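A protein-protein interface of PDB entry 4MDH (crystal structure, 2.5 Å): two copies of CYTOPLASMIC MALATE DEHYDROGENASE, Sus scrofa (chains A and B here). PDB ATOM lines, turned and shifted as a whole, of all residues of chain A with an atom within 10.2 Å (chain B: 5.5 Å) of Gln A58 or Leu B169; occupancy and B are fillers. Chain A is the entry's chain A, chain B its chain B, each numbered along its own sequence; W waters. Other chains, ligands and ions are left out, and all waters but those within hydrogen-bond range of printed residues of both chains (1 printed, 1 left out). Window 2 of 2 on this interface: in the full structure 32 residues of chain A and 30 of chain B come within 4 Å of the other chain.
The side-chain amino group (NZ) of Lys B164 lies close to the backbone carbonyl oxygen (O) of Ser B175, at 3.2 Å.
O of Met A55 lies within hydrogen-bond range of NH2 of Arg B230 (2.8 Å). The side-chain amide oxygen (OE1) of Gln A58 lies within hydrogen-bond range of the guanidinium group (NH2) of Arg B230, at 2.8 Å. NH2 of Arg B230 is in salt-bridge range of OD1 of Asp A59 (3.1 Å).
Water W1 lies within hydrogen-bond range of the side-chain carboxylate of Asp A59 and the side-chain amide oxygen of Gln B166.
Among the printed residues, 7 pairs touch across the chains.
Of the printed residues of chain B, Met A55 touches Arg B230 (2.8 Å). Of chain B, only Ala B165, Leu B169 and Arg B230 come within 4 Å of Gln A58. Printed residues of chain B within 4 Å of Asp A59: Ala B165 and Arg B230. Of the printed residues of chain B, Ala A61 touches Ser B175 (3.4 Å). Of chain A, only Gln A58 and Asp A59 come within 4 Å of Ala B165. No residue of chain A comes within 4 Å of Gln B166. No residue of chain A comes within 4 Å of Ala B168. Printed residues of chain A within 4 Å of Ser B175: Ala A61 (3.4 Å). The nearest residue of chain B that does not touch Gln A58 is Ser B175 (4.5 Å). The nearest residue of chain A that does not touch Leu B169 is Asp A59 (6.0 Å). The nearest printed residue of chain A that does not touch Ser B175 is Gln A58 (4.5 Å).
No position is printed for both chains. Of the 7 pairs that touch across the chains among the printed residues, none has its exchanged pair printed and touching as well.
Ala B165 touches Gln A58. OE1 of Gln A58 touches CD1 of Leu B169, 3.6 Å away. OD1 of Asp A59 touches CB of Ala B165, at 3.4 Å. Ala A61 touches Ser B175.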
ATOM      1  N   LEU A  21      22.420 -16.649  13.676  1.00  0.00           N
ATOM      2  CA  LEU A  21      21.129 -17.263  14.043  1.00  0.00           C
ATOM      3  C   LEU A  21      20.078 -17.349  12.957  1.00  0.00           C
ATOM      4  O   LEU A  21      19.304 -18.313  12.982  1.00  0.00           O
ATOM      5  CB  LEU A  21      20.470 -16.613  15.270  1.00  0.00           C
ATOM      6  CG  LEU A  21      21.153 -16.917  16.586  1.00  0.00           C
ATOM      7  CD1 LEU A  21      20.332 -16.326  17.736  1.00  0.00           C
ATOM      8  CD2 LEU A  21      21.229 -18.403  16.726  1.00  0.00           C
ATOM      9  N   TYR A  22      19.989 -16.311  12.103  1.00  0.00           N
ATOM     10  CA  TYR A  22      19.056 -16.321  10.989  1.00  0.00           C
ATOM     11  C   TYR A  22      19.377 -17.439  10.029  1.00  0.00           C
ATOM     12  O   TYR A  22      18.490 -18.038   9.438  1.00  0.00           O
ATOM     13  CB  TYR A  22      18.846 -14.982  10.239  1.00  0.00           C
ATOM     14  CG  TYR A  22      17.862 -15.100   9.115  1.00  0.00           C
ATOM     15  CD1 TYR A  22      16.497 -15.261   9.377  1.00  0.00           C
ATOM     16  CD2 TYR A  22      18.251 -15.108   7.766  1.00  0.00           C
ATOM     17  CE1 TYR A  22      15.570 -15.446   8.335  1.00  0.00           C
ATOM     18  CE2 TYR A  22      17.347 -15.225   6.710  1.00  0.00           C
ATOM     19  CZ  TYR A  22      15.993 -15.390   7.007  1.00  0.00           C
ATOM     20  OH  TYR A  22      15.075 -15.518   6.022  1.00  0.00           O
ATOM     21  N   GLY A  25      18.416 -21.006  11.611  1.00  0.00           N
ATOM     22  CA  GLY A  25      16.964 -21.067  11.535  1.00  0.00           C
ATOM     23  C   GLY A  25      16.284 -21.327  10.157  1.00  0.00           C
ATOM     24  O   GLY A  25      15.156 -21.815  10.116  1.00  0.00           O
ATOM     25  N   LEU A  38      16.718 -24.833  19.114  1.00  0.00           N
ATOM     26  CA  LEU A  38      17.824 -23.927  19.250  1.00  0.00           C
ATOM     27  C   LEU A  38      18.039 -23.582  20.668  1.00  0.00           C
ATOM     28  O   LEU A  38      17.146 -23.050  21.317  1.00  0.00           O
ATOM     29  CB  LEU A  38      17.664 -22.686  18.340  1.00  0.00           C
ATOM     30  CG  LEU A  38      18.846 -21.701  18.338  1.00  0.00           C
ATOM     31  CD1 LEU A  38      20.134 -22.445  18.020  1.00  0.00           C
ATOM     32  CD2 LEU A  38      18.599 -20.594  17.299  1.00  0.00           C
ATOM     33  N   LEU A  40      20.117 -21.360  23.329  1.00  0.00           N
ATOM     34  CA  LEU A  40      20.963 -20.213  23.340  1.00  0.00           C
ATOM     35  C   LEU A  40      21.576 -19.982  24.723  1.00  0.00           C
ATOM     36  O   LEU A  40      20.874 -20.045  25.734  1.00  0.00           O
ATOM     37  CB  LEU A  40      20.189 -18.994  22.820  1.00  0.00           C
ATOM     38  CG  LEU A  40      19.474 -19.270  21.503  1.00  0.00           C
ATOM     39  CD1 LEU A  40      18.422 -18.179  21.217  1.00  0.00           C
ATOM     40  CD2 LEU A  40      20.494 -19.257  20.358  1.00  0.00           C
ATOM     41  N   LEU A  50      18.587 -11.544  24.821  1.00  0.00           N
ATOM     42  CA  LEU A  50      18.110 -12.789  24.216  1.00  0.00           C
ATOM     43  C   LEU A  50      16.596 -12.818  23.998  1.00  0.00           C
ATOM     44  O   LEU A  50      16.095 -13.397  23.041  1.00  0.00           O
ATOM     45  CB  LEU A  50      18.447 -14.033  25.081  1.00  0.00           C
ATOM     46  CG  LEU A  50      19.905 -14.166  25.476  1.00  0.00           C
ATOM     47  CD1 LEU A  50      20.305 -15.643  25.511  1.00  0.00           C
ATOM     48  CD2 LEU A  50      20.691 -13.385  24.442  1.00  0.00           C
ATOM     49  N   ASP A  51      15.876 -12.315  24.977  1.00  0.00           N
ATOM     50  CA  ASP A  51      14.439 -12.262  24.962  1.00  0.00           C
ATOM     51  C   ASP A  51      14.134 -11.484  23.748  1.00  0.00           C
ATOM     52  O   ASP A  51      13.193 -11.726  23.051  1.00  0.00           O
ATOM     53  CB  ASP A  51      13.948 -11.375  26.145  1.00  0.00           C
ATOM     54  CG  ASP A  51      13.397 -12.032  27.398  1.00  0.00           C
ATOM     55  OD1 ASP A  51      13.020 -13.193  27.416  1.00  0.00           O
ATOM     56  OD2 ASP A  51      13.328 -11.196  28.439  1.00  0.00           O
ATOM     57  N   GLY A  52      14.946 -10.478  23.551  1.00  0.00           N
ATOM     58  CA  GLY A  52      14.801  -9.583  22.445  1.00  0.00           C
ATOM     59  C   GLY A  52      15.016 -10.293  21.158  1.00  0.00           C
ATOM     60  O   GLY A  52      14.189 -10.173  20.258  1.00  0.00           O
ATOM     61  N   VAL A  53      16.109 -11.034  21.094  1.00  0.00           N
ATOM     62  CA  VAL A  53      16.455 -11.838  19.939  1.00  0.00           C
ATOM     63  C   VAL A  53      15.419 -12.961  19.680  1.00  0.00           C
ATOM     64  O   VAL A  53      15.237 -13.405  18.551  1.00  0.00           O
ATOM     65  CB  VAL A  53      17.891 -12.422  20.032  1.00  0.00           C
ATOM     66  CG1 VAL A  53      18.228 -13.273  18.815  1.00  0.00           C
ATOM     67  CG2 VAL A  53      18.954 -11.340  20.247  1.00  0.00           C
ATOM     68  N   LEU A  54      14.754 -13.453  20.719  1.00  0.00           N
ATOM     69  CA  LEU A  54      13.730 -14.470  20.576  1.00  0.00           C
ATOM     70  C   LEU A  54      12.543 -13.844  19.873  1.00  0.00           C
ATOM     71  O   LEU A  54      11.809 -14.453  19.129  1.00  0.00           O
ATOM     72  CB  LEU A  54      13.277 -14.965  21.972  1.00  0.00           C
ATOM     73  CG  LEU A  54      14.264 -15.963  22.615  1.00  0.00           C
ATOM     74  CD1 LEU A  54      13.660 -16.678  23.832  1.00  0.00           C
ATOM     75  CD2 LEU A  54      14.688 -16.999  21.586  1.00  0.00           C
ATOM     76  N   MET A  55      12.374 -12.578  20.130  1.00  0.00           N
ATOM     77  CA  MET A  55      11.311 -11.784  19.566  1.00  0.00           C
ATOM     78  C   MET A  55      11.441 -11.615  18.070  1.00  0.00           C
ATOM     79  O   MET A  55      10.463 -11.678  17.355  1.00  0.00           O
ATOM     80  CB  MET A  55      11.305 -10.418  20.273  1.00  0.00           C
ATOM     81  CG  MET A  55      10.207 -10.334  21.315  1.00  0.00           C
ATOM     82  SD  MET A  55       9.872  -8.630  21.802  1.00  0.00           S
ATOM     83  CE  MET A  55      11.441  -8.304  22.623  1.00  0.00           C
ATOM     84  N   GLU A  56      12.668 -11.337  17.621  1.00  0.00           N
ATOM     85  CA  GLU A  56      12.984 -11.187  16.211  1.00  0.00           C
ATOM     86  C   GLU A  56      12.956 -12.495  15.481  1.00  0.00           C
ATOM     87  O   GLU A  56      12.736 -12.496  14.291  1.00  0.00           O
ATOM     88  CB  GLU A  56      14.360 -10.582  15.953  1.00  0.00           C
ATOM     89  CG  GLU A  56      14.529  -9.107  16.343  1.00  0.00           C
ATOM     90  CD  GLU A  56      15.744  -8.529  15.691  1.00  0.00           C
ATOM     91  OE1 GLU A  56      16.843  -8.659  16.137  1.00  0.00           O
ATOM     92  OE2 GLU A  56      15.512  -7.985  14.539  1.00  0.00           O
ATOM     93  N   LEU A  57      13.224 -13.580  16.192  1.00  0.00           N
ATOM     94  CA  LEU A  57      13.247 -14.898  15.606  1.00  0.00           C
ATOM     95  C   LEU A  57      11.856 -15.319  15.156  1.00  0.00           C
ATOM     96  O   LEU A  57      11.761 -15.991  14.133  1.00  0.00           O
ATOM     97  CB  LEU A  57      14.072 -15.972  16.386  1.00  0.00           C
ATOM     98  CG  LEU A  57      15.624 -15.784  16.310  1.00  0.00           C
ATOM     99  CD1 LEU A  57      16.348 -16.845  17.126  1.00  0.00           C
ATOM    100  CD2 LEU A  57      16.225 -15.730  14.898  1.00  0.00           C
ATOM    101  N   GLN A  58      10.799 -14.851  15.908  1.00  0.00           N
ATOM    102  CA  GLN A  58       9.355 -15.075  15.646  1.00  0.00           C
ATOM    103  C   GLN A  58       8.895 -14.296  14.426  1.00  0.00           C
ATOM    104  O   GLN A  58       8.064 -14.727  13.630  1.00  0.00           O
ATOM    105  CB  GLN A  58       8.428 -14.652  16.838  1.00  0.00           C
ATOM    106  CG  GLN A  58       8.659 -15.323  18.223  1.00  0.00           C
ATOM    107  CD  GLN A  58       7.926 -14.697  19.425  1.00  0.00           C
ATOM    108  OE1 GLN A  58       7.343 -13.591  19.399  1.00  0.00           O
ATOM    109  NE2 GLN A  58       7.966 -15.407  20.546  1.00  0.00           N
ATOM    110  N   ASP A  59       9.436 -13.084  14.338  1.00  0.00           N
ATOM    111  CA  ASP A  59       9.120 -12.148  13.298  1.00  0.00           C
ATOM    112  C   ASP A  59       9.748 -12.527  11.951  1.00  0.00           C
ATOM    113  O   ASP A  59       9.298 -12.066  10.877  1.00  0.00           O
ATOM    114  CB  ASP A  59       9.375 -10.680  13.757  1.00  0.00           C
ATOM    115  CG  ASP A  59       8.393 -10.253  14.833  1.00  0.00           C
ATOM    116  OD1 ASP A  59       7.349 -10.826  15.027  1.00  0.00           O
ATOM    117  OD2 ASP A  59       8.804  -9.257  15.566  1.00  0.00           O
ATOM    118  N   CYS A  60      10.734 -13.448  12.057  1.00  0.00           N
ATOM    119  CA  CYS A  60      11.512 -13.948  10.950  1.00  0.00           C
ATOM    120  C   CYS A  60      10.966 -15.209  10.319  1.00  0.00           C
ATOM    121  O   CYS A  60      11.608 -15.771   9.444  1.00  0.00           O
ATOM    122  CB  CYS A  60      12.991 -14.101  11.330  1.00  0.00           C
ATOM    123  SG  CYS A  60      13.852 -12.518  11.397  1.00  0.00           S
ATOM    124  N   ALA A  61       9.780 -15.622  10.758  1.00  0.00           N
ATOM    125  CA  ALA A  61       9.105 -16.812  10.254  1.00  0.00           C
ATOM    126  C   ALA A  61      10.062 -17.969   9.982  1.00  0.00           C
ATOM    127  O   ALA A  61      10.479 -18.172   8.816  1.00  0.00           O
ATOM    128  CB  ALA A  61       8.340 -16.486   8.977  1.00  0.00           C
ATOM    129  N   LEU A  62      10.476 -18.661  11.054  1.00  0.00           N
ATOM    130  CA  LEU A  62      11.428 -19.767  10.937  1.00  0.00           C
ATOM    131  C   LEU A  62      10.840 -21.078  11.538  1.00  0.00           C
ATOM    132  O   LEU A  62      10.963 -21.399  12.731  1.00  0.00           O
ATOM    133  CB  LEU A  62      12.880 -19.413  11.402  1.00  0.00           C
ATOM    134  CG  LEU A  62      13.467 -18.069  10.928  1.00  0.00           C
ATOM    135  CD1 LEU A  62      14.540 -17.522  11.884  1.00  0.00           C
ATOM    136  CD2 LEU A  62      14.079 -18.149   9.516  1.00  0.00           C
ATOM    137  N   PRO A  63      10.098 -21.789  10.708  1.00  0.00           N
ATOM    138  CA  PRO A  63       9.417 -22.946  11.150  1.00  0.00           C
ATOM    139  C   PRO A  63      10.368 -24.065  11.559  1.00  0.00           C
ATOM    140  O   PRO A  63      10.031 -24.983  12.300  1.00  0.00           O
ATOM    141  CB  PRO A  63       8.524 -23.385  10.006  1.00  0.00           C
ATOM    142  CG  PRO A  63       8.616 -22.334   8.912  1.00  0.00           C
ATOM    143  CD  PRO A  63       9.742 -21.424   9.316  1.00  0.00           C
ATOM    144  N   LEU A  65      12.591 -23.975  13.601  1.00  0.00           N
ATOM    145  CA  LEU A  65      12.820 -23.814  15.030  1.00  0.00           C
ATOM    146  C   LEU A  65      11.723 -24.403  15.915  1.00  0.00           C
ATOM    147  O   LEU A  65      10.848 -23.692  16.409  1.00  0.00           O
ATOM    148  CB  LEU A  65      13.000 -22.342  15.408  1.00  0.00           C
ATOM    149  CG  LEU A  65      14.185 -21.622  14.741  1.00  0.00           C
ATOM    150  CD1 LEU A  65      14.479 -20.353  15.529  1.00  0.00           C
ATOM    151  CD2 LEU A  65      15.445 -22.489  14.677  1.00  0.00           C
ATOM    152  N   ASP A  67      11.817 -24.932  18.796  1.00  0.00           N
ATOM    153  CA  ASP A  67      11.933 -24.390  20.108  1.00  0.00           C
ATOM    154  C   ASP A  67      13.169 -23.563  20.199  1.00  0.00           C
ATOM    155  O   ASP A  67      14.147 -23.879  19.501  1.00  0.00           O
ATOM    156  CB  ASP A  67      12.029 -25.535  21.151  1.00  0.00           C
ATOM    157  CG  ASP A  67      11.628 -25.139  22.584  1.00  0.00           C
ATOM    158  OD1 ASP A  67      11.810 -25.843  23.577  1.00  0.00           O
ATOM    159  OD2 ASP A  67      11.037 -23.956  22.676  1.00  0.00           O
ATOM    160  N   VAL A  68      13.058 -22.490  21.042  1.00  0.00           N
ATOM    161  CA  VAL A  68      14.117 -21.575  21.326  1.00  0.00           C
ATOM    162  C   VAL A  68      14.275 -21.348  22.804  1.00  0.00           C
ATOM    163  O   VAL A  68      13.438 -20.672  23.414  1.00  0.00           O
ATOM    164  CB  VAL A  68      14.093 -20.311  20.518  1.00  0.00           C
ATOM    165  CG1 VAL A  68      15.504 -19.734  20.474  1.00  0.00           C
ATOM    166  CG2 VAL A  68      13.648 -20.626  19.105  1.00  0.00           C
ATOM    167  N   LYS B 164       1.404 -11.056  10.880  1.00  0.00           N
ATOM    168  CA  LYS B 164       1.370 -12.473  10.567  1.00  0.00           C
ATOM    169  C   LYS B 164       1.948 -13.331  11.691  1.00  0.00           C
ATOM    170  O   LYS B 164       1.496 -14.456  11.918  1.00  0.00           O
ATOM    171  CB  LYS B 164       2.265 -12.727   9.377  1.00  0.00           C
ATOM    172  CG  LYS B 164       1.715 -12.307   8.057  1.00  0.00           C
ATOM    173  CD  LYS B 164       2.688 -12.745   6.983  1.00  0.00           C
ATOM    174  CE  LYS B 164       2.437 -14.159   6.548  1.00  0.00           C
ATOM    175  NZ  LYS B 164       3.589 -14.728   5.878  1.00  0.00           N
ATOM    176  N   ALA B 165       3.023 -12.835  12.324  1.00  0.00           N
ATOM    177  CA  ALA B 165       3.645 -13.556  13.397  1.00  0.00           C
ATOM    178  C   ALA B 165       2.759 -13.529  14.596  1.00  0.00           C
ATOM    179  O   ALA B 165       2.729 -14.495  15.351  1.00  0.00           O
ATOM    180  CB  ALA B 165       4.992 -12.992  13.768  1.00  0.00           C
ATOM    181  N   GLN B 166       2.048 -12.410  14.753  1.00  0.00           N
ATOM    182  CA  GLN B 166       1.093 -12.245  15.834  1.00  0.00           C
ATOM    183  C   GLN B 166      -0.117 -13.199  15.676  1.00  0.00           C
ATOM    184  O   GLN B 166      -0.635 -13.834  16.593  1.00  0.00           O
ATOM    185  CB  GLN B 166       0.650 -10.771  16.003  1.00  0.00           C
ATOM    186  CG  GLN B 166       1.607  -9.900  16.865  1.00  0.00           C
ATOM    187  CD  GLN B 166       2.192 -10.590  18.068  1.00  0.00           C
ATOM    188  OE1 GLN B 166       3.411 -10.797  18.171  1.00  0.00           O
ATOM    189  NE2 GLN B 166       1.330 -10.912  19.020  1.00  0.00           N
ATOM    190  N   ILE B 167      -0.565 -13.307  14.475  1.00  0.00           N
ATOM    191  CA  ILE B 167      -1.678 -14.128  14.221  1.00  0.00           C
ATOM    192  C   ILE B 167      -1.341 -15.569  14.520  1.00  0.00           C
ATOM    193  O   ILE B 167      -2.019 -16.199  15.303  1.00  0.00           O
ATOM    194  CB  ILE B 167      -2.246 -13.826  12.841  1.00  0.00           C
ATOM    195  CG1 ILE B 167      -2.722 -12.370  12.826  1.00  0.00           C
ATOM    196  CG2 ILE B 167      -3.372 -14.787  12.439  1.00  0.00           C
ATOM    197  CD1 ILE B 167      -4.193 -12.186  13.188  1.00  0.00           C
ATOM    198  N   ALA B 168      -0.272 -16.054  13.940  1.00  0.00           N
ATOM    199  CA  ALA B 168       0.223 -17.389  14.153  1.00  0.00           C
ATOM    200  C   ALA B 168       0.299 -17.720  15.627  1.00  0.00           C
ATOM    201  O   ALA B 168      -0.158 -18.773  16.063  1.00  0.00           O
ATOM    202  CB  ALA B 168       1.614 -17.488  13.569  1.00  0.00           C
ATOM    203  N   LEU B 169       0.904 -16.810  16.407  1.00  0.00           N
ATOM    204  CA  LEU B 169       1.067 -17.016  17.839  1.00  0.00           C
ATOM    205  C   LEU B 169      -0.228 -17.390  18.496  1.00  0.00           C
ATOM    206  O   LEU B 169      -0.337 -18.468  19.104  1.00  0.00           O
ATOM    207  CB  LEU B 169       1.867 -15.907  18.548  1.00  0.00           C
ATOM    208  CG  LEU B 169       3.322 -16.002  18.078  1.00  0.00           C
ATOM    209  CD1 LEU B 169       4.101 -14.696  18.190  1.00  0.00           C
ATOM    210  CD2 LEU B 169       4.036 -17.138  18.769  1.00  0.00           C
ATOM    211  N   LYS B 170      -1.205 -16.501  18.259  1.00  0.00           N
ATOM    212  CA  LYS B 170      -2.569 -16.619  18.738  1.00  0.00           C
ATOM    213  C   LYS B 170      -3.203 -17.988  18.483  1.00  0.00           C
ATOM    214  O   LYS B 170      -3.597 -18.680  19.410  1.00  0.00           O
ATOM    215  CB  LYS B 170      -3.440 -15.436  18.293  1.00  0.00           C
ATOM    216  CG  LYS B 170      -4.861 -15.456  18.825  1.00  0.00           C
ATOM    217  CD  LYS B 170      -5.056 -14.740  20.162  1.00  0.00           C
ATOM    218  CE  LYS B 170      -6.509 -14.289  20.333  1.00  0.00           C
ATOM    219  NZ  LYS B 170      -7.011 -14.250  21.721  1.00  0.00           N
ATOM    220  N   LEU B 171      -3.272 -18.377  17.232  1.00  0.00           N
ATOM    221  CA  LEU B 171      -3.957 -19.586  16.772  1.00  0.00           C
ATOM    222  C   LEU B 171      -3.121 -20.828  16.831  1.00  0.00           C
ATOM    223  O   LEU B 171      -3.612 -21.937  16.635  1.00  0.00           O
ATOM    224  CB  LEU B 171      -4.594 -19.382  15.357  1.00  0.00           C
ATOM    225  CG  LEU B 171      -5.264 -17.995  15.201  1.00  0.00           C
ATOM    226  CD1 LEU B 171      -5.498 -17.615  13.736  1.00  0.00           C
ATOM    227  CD2 LEU B 171      -6.539 -17.862  16.032  1.00  0.00           C
ATOM    228  N   GLY B 172      -1.847 -20.628  17.111  1.00  0.00           N
ATOM    229  CA  GLY B 172      -0.920 -21.732  17.227  1.00  0.00           C
ATOM    230  C   GLY B 172      -0.596 -22.429  15.915  1.00  0.00           C
ATOM    231  O   GLY B 172      -0.410 -23.634  15.868  1.00  0.00           O
ATOM    232  N   VAL B 173      -0.510 -21.656  14.861  1.00  0.00           N
ATOM    233  CA  VAL B 173      -0.120 -22.144  13.555  1.00  0.00           C
ATOM    234  C   VAL B 173       1.171 -21.475  13.125  1.00  0.00           C
ATOM    235  O   VAL B 173       1.895 -20.837  13.872  1.00  0.00           O
ATOM    236  CB  VAL B 173      -1.152 -21.834  12.497  1.00  0.00           C
ATOM    237  CG1 VAL B 173      -2.399 -22.659  12.670  1.00  0.00           C
ATOM    238  CG2 VAL B 173      -1.459 -20.366  12.643  1.00  0.00           C
ATOM    239  N   SER B 175       3.458 -18.759  10.787  1.00  0.00           N
ATOM    240  CA  SER B 175       3.240 -17.520  10.107  1.00  0.00           C
ATOM    241  C   SER B 175       3.095 -17.734   8.624  1.00  0.00           C
ATOM    242  O   SER B 175       2.546 -16.917   7.941  1.00  0.00           O
ATOM    243  CB  SER B 175       4.177 -16.395  10.484  1.00  0.00           C
ATOM    244  OG  SER B 175       5.450 -16.924  10.720  1.00  0.00           O
ATOM    245  N   ARG B 230       5.740  -3.339  18.651  1.00  0.00           N
ATOM    246  CA  ARG B 230       6.822  -4.203  18.213  1.00  0.00           C
ATOM    247  C   ARG B 230       8.235  -3.617  17.984  1.00  0.00           C
ATOM    248  O   ARG B 230       9.187  -4.104  18.541  1.00  0.00           O
ATOM    249  CB  ARG B 230       6.382  -5.368  17.278  1.00  0.00           C
ATOM    250  CG  ARG B 230       7.440  -6.475  16.997  1.00  0.00           C
ATOM    251  CD  ARG B 230       7.731  -7.439  18.144  1.00  0.00           C
ATOM    252  NE  ARG B 230       7.981  -8.824  17.759  1.00  0.00           N
ATOM    253  CZ  ARG B 230       7.500  -9.892  18.455  1.00  0.00           C
ATOM    254  NH1 ARG B 230       6.723  -9.733  19.507  1.00  0.00           N
ATOM    255  NH2 ARG B 230       7.781 -11.154  18.097  1.00  0.00           N
HETATM  256  O   HOH W   1       5.092  -9.576  15.859  1.00  0.00           O
